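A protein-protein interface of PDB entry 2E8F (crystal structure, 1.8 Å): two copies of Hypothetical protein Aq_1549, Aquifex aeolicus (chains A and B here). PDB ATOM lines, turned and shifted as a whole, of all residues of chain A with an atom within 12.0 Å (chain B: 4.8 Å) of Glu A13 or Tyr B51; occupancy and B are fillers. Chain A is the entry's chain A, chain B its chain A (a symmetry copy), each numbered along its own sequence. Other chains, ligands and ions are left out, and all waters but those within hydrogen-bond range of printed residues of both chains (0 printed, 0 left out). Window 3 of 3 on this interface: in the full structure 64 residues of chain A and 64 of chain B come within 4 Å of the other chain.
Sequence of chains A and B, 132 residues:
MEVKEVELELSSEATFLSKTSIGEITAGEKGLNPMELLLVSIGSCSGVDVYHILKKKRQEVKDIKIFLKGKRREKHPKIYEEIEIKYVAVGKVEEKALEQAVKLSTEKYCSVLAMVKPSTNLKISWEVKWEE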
ATOM      1  N   LEU A   8      -2.069  18.989 -13.107  1.00  0.00           N
ATOM      2  CA  LEU A   8      -1.477  17.887 -13.850  1.00  0.00           C
ATOM      3  C   LEU A   8      -2.190  17.667 -15.171  1.00  0.00           C
ATOM      4  O   LEU A   8      -3.384  17.933 -15.295  1.00  0.00           O
ATOM      5  CB  LEU A   8      -1.552  16.585 -13.045  1.00  0.00           C
ATOM      6  CG  LEU A   8      -0.592  16.368 -11.871  1.00  0.00           C
ATOM      7  CD1 LEU A   8      -0.743  17.471 -10.846  1.00  0.00           C
ATOM      8  CD2 LEU A   8      -0.878  15.013 -11.252  1.00  0.00           C
ATOM      9  N   GLU A   9      -1.442  17.175 -16.149  1.00  0.00           N
ATOM     10  CA  GLU A   9      -1.979  16.878 -17.469  1.00  0.00           C
ATOM     11  C   GLU A   9      -1.238  15.660 -17.993  1.00  0.00           C
ATOM     12  O   GLU A   9      -0.034  15.515 -17.785  1.00  0.00           O
ATOM     13  CB  GLU A   9      -1.786  18.073 -18.405  1.00  0.00           C
ATOM     14  CG  GLU A   9      -2.236  17.835 -19.830  1.00  0.00           C
ATOM     15  CD  GLU A   9      -2.350  19.126 -20.618  1.00  0.00           C
ATOM     16  OE1 GLU A   9      -1.445  19.982 -20.494  1.00  0.00           O
ATOM     17  OE2 GLU A   9      -3.341  19.283 -21.363  1.00  0.00           O
ATOM     18  N   LEU A  10      -1.968  14.770 -18.655  1.00  0.00           N
ATOM     19  CA  LEU A  10      -1.380  13.557 -19.197  1.00  0.00           C
ATOM     20  C   LEU A  10      -0.237  13.931 -20.153  1.00  0.00           C
ATOM     21  O   LEU A  10      -0.381  14.836 -20.977  1.00  0.00           O
ATOM     22  CB  LEU A  10      -2.471  12.757 -19.917  1.00  0.00           C
ATOM     23  CG  LEU A  10      -2.278  11.267 -20.190  1.00  0.00           C
ATOM     24  CD1 LEU A  10      -2.072  10.510 -18.881  1.00  0.00           C
ATOM     25  CD2 LEU A  10      -3.513  10.742 -20.921  1.00  0.00           C
ATOM     26  N   SER A  11       0.894  13.238 -20.026  1.00  0.00           N
ATOM     27  CA  SER A  11       2.075  13.492 -20.854  1.00  0.00           C
ATOM     28  C   SER A  11       2.484  12.258 -21.661  1.00  0.00           C
ATOM     29  O   SER A  11       3.073  12.373 -22.735  1.00  0.00           O
ATOM     30  CB  SER A  11       3.241  13.932 -19.969  1.00  0.00           C
ATOM     31  OG  SER A  11       3.487  12.969 -18.957  1.00  0.00           O
ATOM     32  N   SER A  12       2.190  11.085 -21.114  1.00  0.00           N
ATOM     33  CA  SER A  12       2.471   9.809 -21.760  1.00  0.00           C
ATOM     34  C   SER A  12       1.587   8.795 -21.042  1.00  0.00           C
ATOM     35  O   SER A  12       0.839   9.167 -20.139  1.00  0.00           O
ATOM     36  CB  SER A  12       3.953   9.432 -21.631  1.00  0.00           C
ATOM     37  OG  SER A  12       4.315   9.155 -20.290  1.00  0.00           O
ATOM     38  N   GLU A  13       1.659   7.527 -21.436  1.00  0.00           N
ATOM     39  CA  GLU A  13       0.829   6.499 -20.813  1.00  0.00           C
ATOM     40  C   GLU A  13       0.868   6.539 -19.288  1.00  0.00           C
ATOM     41  O   GLU A  13       1.917   6.329 -18.678  1.00  0.00           O
ATOM     42  CB  GLU A  13       1.246   5.104 -21.297  1.00  0.00           C
ATOM     43  CG  GLU A  13       0.427   3.966 -20.699  1.00  0.00           C
ATOM     44  CD  GLU A  13       0.720   2.624 -21.348  1.00  0.00           C
ATOM     45  OE1 GLU A  13       1.900   2.208 -21.358  1.00  0.00           O
ATOM     46  OE2 GLU A  13      -0.234   1.982 -21.847  1.00  0.00           O
ATOM     47  N   ALA A  14      -0.286   6.814 -18.689  1.00  0.00           N
ATOM     48  CA  ALA A  14      -0.429   6.872 -17.237  1.00  0.00           C
ATOM     49  C   ALA A  14       0.652   7.719 -16.575  1.00  0.00           C
ATOM     50  O   ALA A  14       1.134   7.387 -15.490  1.00  0.00           O
ATOM     51  CB  ALA A  14      -0.411   5.456 -16.660  1.00  0.00           C
ATOM     52  N   THR A  15       1.018   8.818 -17.226  1.00  0.00           N
ATOM     53  CA  THR A  15       2.043   9.719 -16.706  1.00  0.00           C
ATOM     54  C   THR A  15       1.568  11.156 -16.866  1.00  0.00           C
ATOM     55  O   THR A  15       0.907  11.482 -17.846  1.00  0.00           O
ATOM     56  CB  THR A  15       3.367   9.513 -17.452  1.00  0.00           C
ATOM     57  OG1 THR A  15       3.666   8.113 -17.484  1.00  0.00           O
ATOM     58  CG2 THR A  15       4.493  10.242 -16.744  1.00  0.00           C
ATOM     59  N   PHE A  16       1.907  12.014 -15.905  1.00  0.00           N
ATOM     60  CA  PHE A  16       1.458  13.404 -15.932  1.00  0.00           C
ATOM     61  C   PHE A  16       2.522  14.472 -15.794  1.00  0.00           C
ATOM     62  O   PHE A  16       3.427  14.344 -14.973  1.00  0.00           O
ATOM     63  CB  PHE A  16       0.453  13.637 -14.803  1.00  0.00           C
ATOM     64  CG  PHE A  16      -0.735  12.741 -14.871  1.00  0.00           C
ATOM     65  CD1 PHE A  16      -0.669  11.449 -14.366  1.00  0.00           C
ATOM     66  CD2 PHE A  16      -1.905  13.166 -15.489  1.00  0.00           C
ATOM     67  CE1 PHE A  16      -1.749  10.587 -14.480  1.00  0.00           C
ATOM     68  CE2 PHE A  16      -2.995  12.312 -15.607  1.00  0.00           C
ATOM     69  CZ  PHE A  16      -2.917  11.024 -15.103  1.00  0.00           C
ATOM     70  N   LEU A  17       2.393  15.527 -16.592  1.00  0.00           N
ATOM     71  CA  LEU A  17       3.290  16.667 -16.487  1.00  0.00           C
ATOM     72  C   LEU A  17       2.611  17.470 -15.386  1.00  0.00           C
ATOM     73  O   LEU A  17       1.445  17.867 -15.511  1.00  0.00           O
ATOM     74  CB  LEU A  17       3.348  17.449 -17.802  1.00  0.00           C
ATOM     75  CG  LEU A  17       4.573  17.077 -18.647  1.00  0.00           C
ATOM     76  CD1 LEU A  17       4.471  17.679 -20.044  1.00  0.00           C
ATOM     77  CD2 LEU A  17       5.831  17.568 -17.938  1.00  0.00           C
ATOM     78  N   SER A  18       3.340  17.681 -14.298  1.00  0.00           N
ATOM     79  CA  SER A  18       2.801  18.358 -13.133  1.00  0.00           C
ATOM     80  C   SER A  18       3.389  19.743 -12.924  1.00  0.00           C
ATOM     81  O   SER A  18       4.585  19.888 -12.676  1.00  0.00           O
ATOM     82  CB  SER A  18       3.053  17.487 -11.907  1.00  0.00           C
ATOM     83  OG  SER A  18       2.826  16.120 -12.222  1.00  0.00           O
ATOM     84  N   THR A  26       7.553  15.295 -14.513  1.00  0.00           N
ATOM     85  CA  THR A  26       6.658  14.228 -14.929  1.00  0.00           C
ATOM     86  C   THR A  26       6.548  13.225 -13.803  1.00  0.00           C
ATOM     87  O   THR A  26       7.554  12.742 -13.283  1.00  0.00           O
ATOM     88  CB  THR A  26       7.155  13.513 -16.200  1.00  0.00           C
ATOM     89  OG1 THR A  26       8.485  13.020 -15.990  1.00  0.00           O
ATOM     90  CG2 THR A  26       7.137  14.468 -17.381  1.00  0.00           C
ATOM     91  N   ALA A  27       5.315  12.927 -13.417  1.00  0.00           N
ATOM     92  CA  ALA A  27       5.063  11.987 -12.337  1.00  0.00           C
ATOM     93  C   ALA A  27       4.094  10.910 -12.809  1.00  0.00           C
ATOM     94  O   ALA A  27       3.064  11.212 -13.413  1.00  0.00           O
ATOM     95  CB  ALA A  27       4.481  12.725 -11.137  1.00  0.00           C
ATOM     96  N   GLY A  28       4.430   9.658 -12.533  1.00  0.00           N
ATOM     97  CA  GLY A  28       3.567   8.569 -12.940  1.00  0.00           C
ATOM     98  C   GLY A  28       4.313   7.334 -13.392  1.00  0.00           C
ATOM     99  O   GLY A  28       5.472   7.121 -13.047  1.00  0.00           O
ATOM    100  N   GLU A  29       3.630   6.520 -14.185  1.00  0.00           N
ATOM    101  CA  GLU A  29       4.174   5.270 -14.693  1.00  0.00           C
ATOM    102  C   GLU A  29       5.510   5.409 -15.430  1.00  0.00           C
ATOM    103  O   GLU A  29       6.433   4.619 -15.213  1.00  0.00           O
ATOM    104  CB  GLU A  29       3.127   4.636 -15.600  1.00  0.00           C
ATOM    105  CG  GLU A  29       3.320   3.178 -15.882  1.00  0.00           C
ATOM    106  CD  GLU A  29       2.006   2.510 -16.201  1.00  0.00           C
ATOM    107  OE1 GLU A  29       1.168   2.396 -15.281  1.00  0.00           O
ATOM    108  OE2 GLU A  29       1.807   2.112 -17.365  1.00  0.00           O
ATOM    109  N   LYS A  30       5.619   6.411 -16.298  1.00  0.00           N
ATOM    110  CA  LYS A  30       6.850   6.621 -17.053  1.00  0.00           C
ATOM    111  C   LYS A  30       7.647   7.817 -16.548  1.00  0.00           C
ATOM    112  O   LYS A  30       8.568   8.285 -17.216  1.00  0.00           O
ATOM    113  CB  LYS A  30       6.534   6.807 -18.540  1.00  0.00           C
ATOM    114  CG  LYS A  30       5.851   5.610 -19.168  1.00  0.00           C
ATOM    115  CD  LYS A  30       5.722   5.772 -20.671  1.00  0.00           C
ATOM    116  CE  LYS A  30       5.069   4.552 -21.297  1.00  0.00           C
ATOM    117  NZ  LYS A  30       5.010   4.667 -22.779  1.00  0.00           N
ATOM    118  N   GLY A  31       7.283   8.313 -15.372  1.00  0.00           N
ATOM    119  CA  GLY A  31       7.981   9.451 -14.799  1.00  0.00           C
ATOM    120  C   GLY A  31       8.354   9.155 -13.361  1.00  0.00           C
ATOM    121  O   GLY A  31       8.628   8.006 -13.017  1.00  0.00           O
ATOM    122  N   LEU A  32       8.371  10.182 -12.519  1.00  0.00           N
ATOM    123  CA  LEU A  32       8.702   9.995 -11.110  1.00  0.00           C
ATOM    124  C   LEU A  32       7.607   9.159 -10.460  1.00  0.00           C
ATOM    125  O   LEU A  32       6.427   9.464 -10.611  1.00  0.00           O
ATOM    126  CB  LEU A  32       8.788  11.349 -10.408  1.00  0.00           C
ATOM    127  CG  LEU A  32       9.907  12.300 -10.834  1.00  0.00           C
ATOM    128  CD1 LEU A  32       9.505  13.735 -10.535  1.00  0.00           C
ATOM    129  CD2 LEU A  32      11.194  11.919 -10.112  1.00  0.00           C
ATOM    130  N   ASN A  33       7.994   8.111  -9.743  1.00  0.00           N
ATOM    131  CA  ASN A  33       7.023   7.252  -9.072  1.00  0.00           C
ATOM    132  C   ASN A  33       6.296   8.055  -7.991  1.00  0.00           C
ATOM    133  O   ASN A  33       6.932   8.656  -7.128  1.00  0.00           O
ATOM    134  CB  ASN A  33       7.735   6.049  -8.453  1.00  0.00           C
ATOM    135  CG  ASN A  33       6.793   5.158  -7.684  1.00  0.00           C
ATOM    136  OD1 ASN A  33       6.723   5.218  -6.457  1.00  0.00           O
ATOM    137  ND2 ASN A  33       6.038   4.334  -8.408  1.00  0.00           N
ATOM    138  N   PRO A  34       4.951   8.069  -8.019  1.00  0.00           N
ATOM    139  CA  PRO A  34       4.194   8.829  -7.015  1.00  0.00           C
ATOM    140  C   PRO A  34       4.512   8.518  -5.551  1.00  0.00           C
ATOM    141  O   PRO A  34       4.647   9.436  -4.737  1.00  0.00           O
ATOM    142  CB  PRO A  34       2.742   8.533  -7.384  1.00  0.00           C
ATOM    143  CG  PRO A  34       2.817   8.388  -8.884  1.00  0.00           C
ATOM    144  CD  PRO A  34       4.050   7.524  -9.050  1.00  0.00           C
ATOM    145  N   GLY B  47      -4.078   9.777 -10.570  1.00  0.00           N
ATOM    146  CA  GLY B  47      -4.141   9.889 -12.016  1.00  0.00           C
ATOM    147  C   GLY B  47      -3.794   8.582 -12.707  1.00  0.00           C
ATOM    148  O   GLY B  47      -4.385   8.238 -13.734  1.00  0.00           O
ATOM    149  N   VAL B  48      -2.827   7.858 -12.155  1.00  0.00           N
ATOM    150  CA  VAL B  48      -2.427   6.574 -12.716  1.00  0.00           C
ATOM    151  C   VAL B  48      -3.608   5.604 -12.633  1.00  0.00           C
ATOM    152  O   VAL B  48      -3.880   4.876 -13.584  1.00  0.00           O
ATOM    153  CB  VAL B  48      -1.226   5.981 -11.954  1.00  0.00           C
ATOM    154  CG1 VAL B  48      -0.969   4.544 -12.403  1.00  0.00           C
ATOM    155  CG2 VAL B  48       0.014   6.828 -12.209  1.00  0.00           C
ATOM    156  N   ASP B  49      -4.306   5.610 -11.497  1.00  0.00           N
ATOM    157  CA  ASP B  49      -5.471   4.733 -11.306  1.00  0.00           C
ATOM    158  C   ASP B  49      -6.556   5.064 -12.318  1.00  0.00           C
ATOM    159  O   ASP B  49      -7.055   4.190 -13.029  1.00  0.00           O
ATOM    160  CB  ASP B  49      -6.095   4.901  -9.915  1.00  0.00           C
ATOM    161  CG  ASP B  49      -5.167   4.507  -8.786  1.00  0.00           C
ATOM    162  OD1 ASP B  49      -4.363   3.563  -8.947  1.00  0.00           O
ATOM    163  OD2 ASP B  49      -5.270   5.138  -7.714  1.00  0.00           O
ATOM    164  N   VAL B  50      -6.937   6.336 -12.358  1.00  0.00           N
ATOM    165  CA  VAL B  50      -7.984   6.789 -13.264  1.00  0.00           C
ATOM    166  C   VAL B  50      -7.656   6.455 -14.715  1.00  0.00           C
ATOM    167  O   VAL B  50      -8.533   6.028 -15.473  1.00  0.00           O
ATOM    168  CB  VAL B  50      -8.220   8.309 -13.111  1.00  0.00           C
ATOM    169  CG1 VAL B  50      -9.245   8.791 -14.134  1.00  0.00           C
ATOM    170  CG2 VAL B  50      -8.715   8.608 -11.706  1.00  0.00           C
ATOM    171  N   TYR B  51      -6.396   6.637 -15.101  1.00  0.00           N
ATOM    172  CA  TYR B  51      -5.980   6.336 -16.468  1.00  0.00           C
ATOM    173  C   TYR B  51      -6.226   4.867 -16.803  1.00  0.00           C
ATOM    174  O   TYR B  51      -6.871   4.545 -17.807  1.00  0.00           O
ATOM    175  CB  TYR B  51      -4.497   6.636 -16.669  1.00  0.00           C
ATOM    176  CG  TYR B  51      -4.012   6.313 -18.062  1.00  0.00           C
ATOM    177  CD1 TYR B  51      -4.127   7.240 -19.098  1.00  0.00           C
ATOM    178  CD2 TYR B  51      -3.458   5.064 -18.353  1.00  0.00           C
ATOM    179  CE1 TYR B  51      -3.698   6.929 -20.394  1.00  0.00           C
ATOM    180  CE2 TYR B  51      -3.031   4.745 -19.637  1.00  0.00           C
ATOM    181  CZ  TYR B  51      -3.151   5.680 -20.653  1.00  0.00           C
ATOM    182  OH  TYR B  51      -2.707   5.360 -21.920  1.00  0.00           O
ATOM    183  N   HIS B  52      -5.708   3.978 -15.964  1.00  0.00           N
ATOM    184  CA  HIS B  52      -5.871   2.545 -16.189  1.00  0.00           C
ATOM    185  C   HIS B  52      -7.323   2.081 -16.142  1.00  0.00           C
ATOM    186  O   HIS B  52      -7.737   1.265 -16.963  1.00  0.00           O
ATOM    187  CB  HIS B  52      -5.043   1.752 -15.177  1.00  0.00           C
ATOM    188  CG  HIS B  52      -3.569   1.851 -15.400  1.00  0.00           C
ATOM    189  ND1 HIS B  52      -2.980   1.548 -16.608  1.00  0.00           N
ATOM    190  CD2 HIS B  52      -2.563   2.221 -14.572  1.00  0.00           C
ATOM    191  CE1 HIS B  52      -1.674   1.729 -16.516  1.00  0.00           C
ATOM    192  NE2 HIS B  52      -1.396   2.137 -15.291  1.00  0.00           N
ATOM    193  N   ILE B  53      -8.091   2.599 -15.188  1.00  0.00           N
ATOM    194  CA  ILE B  53      -9.495   2.222 -15.060  1.00  0.00           C
ATOM    195  C   ILE B  53     -10.286   2.684 -16.281  1.00  0.00           C
ATOM    196  O   ILE B  53     -11.063   1.914 -16.852  1.00  0.00           O
ATOM    197  CB  ILE B  53     -10.135   2.821 -13.784  1.00  0.00           C
ATOM    198  CG1 ILE B  53      -9.485   2.203 -12.543  1.00  0.00           C
ATOM    199  CG2 ILE B  53     -11.640   2.566 -13.773  1.00  0.00           C
ATOM    200  CD1 ILE B  53      -9.904   2.836 -11.226  1.00  0.00           C
ATOM    201  N   LEU B  54     -10.080   3.930 -16.689  1.00  0.00           N
ATOM    202  CA  LEU B  54     -10.772   4.457 -17.860  1.00  0.00           C
ATOM    203  C   LEU B  54     -10.450   3.611 -19.087  1.00  0.00           C
ATOM    204  O   LEU B  54     -11.319   3.356 -19.922  1.00  0.00           O
ATOM    205  CB  LEU B  54     -10.368   5.913 -18.120  1.00  0.00           C
ATOM    206  CG  LEU B  54     -10.993   6.966 -17.203  1.00  0.00           C
ATOM    207  CD1 LEU B  54     -10.531   8.352 -17.630  1.00  0.00           C
ATOM    208  CD2 LEU B  54     -12.508   6.863 -17.274  1.00  0.00           C
ATOM    209  N   LYS B  55      -9.198   3.176 -19.188  1.00  0.00           N
ATOM    210  CA  LYS B  55      -8.766   2.353 -20.307  1.00  0.00           C
ATOM    211  C   LYS B  55      -9.454   0.989 -20.225  1.00  0.00           C
ATOM    212  O   LYS B  55      -9.927   0.458 -21.232  1.00  0.00           O
ATOM    213  CB  LYS B  55      -7.241   2.197 -20.276  1.00  0.00           C
ATOM    214  CG  LYS B  55      -6.645   1.427 -21.439  1.00  0.00           C
ATOM    215  CD  LYS B  55      -5.133   1.631 -21.501  1.00  0.00           C
ATOM    216  CE  LYS B  55      -4.489   0.790 -22.598  1.00  0.00           C
ATOM    217  NZ  LYS B  55      -4.526  -0.669 -22.285  1.00  0.00           N
ATOM    218  N   ILE B  64      -6.205  13.894 -19.662  1.00  0.00           N
ATOM    219  CA  ILE B  64      -6.734  13.850 -18.309  1.00  0.00           C
ATOM    220  C   ILE B  64      -6.061  14.992 -17.564  1.00  0.00           C
ATOM    221  O   ILE B  64      -4.833  15.063 -17.501  1.00  0.00           O
ATOM    222  CB  ILE B  64      -6.400  12.520 -17.597  1.00  0.00           C
ATOM    223  CG1 ILE B  64      -7.108  11.358 -18.297  1.00  0.00           C
ATOM    224  CG2 ILE B  64      -6.828  12.589 -16.134  1.00  0.00           C
ATOM    225  CD1 ILE B  64      -6.753   9.997 -17.730  1.00  0.00           C
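The backbone NH of Leu A10 lies within hydrogen-bond range of the backbone carbonyl oxygen of Ile B64 (3.1 Å). The side-chain carboxylate (OE1) of Glu A29 lies within hydrogen-bond range of a ring nitrogen (NE2) of His B52.
O of Glu A13 is in hydrogen-bond range of OG1 of Thr A15 (2.8 Å). The backbone NH (N) of Leu A17 lies within hydrogen-bond range of the backbone carbonyl oxygen (O) of Glu A9 (2.7 Å). OG of Ser A18 lies within hydrogen-bond range of O of Phe A16, 3.3 Å away. The backbone NH (N) of Glu A29 is in hydrogen-bond range of the backbone carbonyl oxygen (O) of Ala A14, 2.9 Å away. N of Ala A27 sits at hydrogen-bond distance from O of Phe A16 (2.8 Å).
Leu A8 touches Ile B64. O of Ile B64 touches CA of Glu A9, at 3.4 Å. Leu A10 touches Tyr B51 (CD2 to CE1, 3.9 Å). Tyr B51 touches Glu A13 (OH to CG, 3.6 Å). Val B48 touches Ala A14 (CG2 to O, 3.5 Å). CB of Ala A14 touches CD2 of Tyr B51 (3.5 Å). NE2 of His B52 touches CB of Ala A14 (3.7 Å). Gly B47 touches Phe A16 (C to CE1, 3.4 Å). CE1 of Phe A16 touches N of Val B48, at 3.7 Å. Ile B64 touches Phe A16.
Glu A13 touches just one residue of chain B: Tyr B51. Of the printed residues of chain A, Gly B47 touches Phe A16 (3.4 Å). No residue of chain A comes within 4 Å of Asp B49. No residue of chain A comes within 4 Å of Val B50. Of chain A, only Ala A14 and Glu A29 come within 4 Å of His B52. Ile B53 touches none of the printed residues of chain A. No residue of chain A comes within 4 Å of Leu B54. No residue of chain A comes within 4 Å of Lys B55. Printed residues of chain B within 4 Å of Ala A14: Val B48 (3.5 Å), Tyr B51 (3.5 Å) and His B52 (3.7 Å). Printed residues of chain B within 4 Å of Leu A10: Tyr B51 (3.9 Å) and Ile B64 (3.1 Å). Of the printed residues of chain B, Glu A9 touches Ile B64. Of the printed residues of chain B, Phe A16 touches Gly B47 (3.4 Å), Val B48 (3.7 Å) and Ile B64 (3.8 Å). Thr A26 touches none of the printed residues of chain B. The nearest residue of chain A that does not touch Tyr B51 is Phe A16 (4.9 Å).
Of the 10 printed residues of chain B, 5 touch a printed residue of chain A. Along chain B the printed residues that touch a printed residue of chain A span positions 47 to 64. Of the 20 printed residues of chain A, 7 touch a printed residue of chain B. Printed residues of chain A that touch a printed residue of chain B: Leu A8, Glu A9, Leu A10, Glu A13, Ala A14, Phe A16 and Glu A29. Hydrophobic or aromatic side chains of chain A within 4 Å of the printed part of chain B: Leu A10, Ala A14 and Phe A16. Among the printed residues, 12 pairs touch across the chains. Among the printed residues, no Asp or Glu carboxylate lies within 4 Å of a Lys or Arg side-chain nitrogen of the other chain.
No position is printed for both chains.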
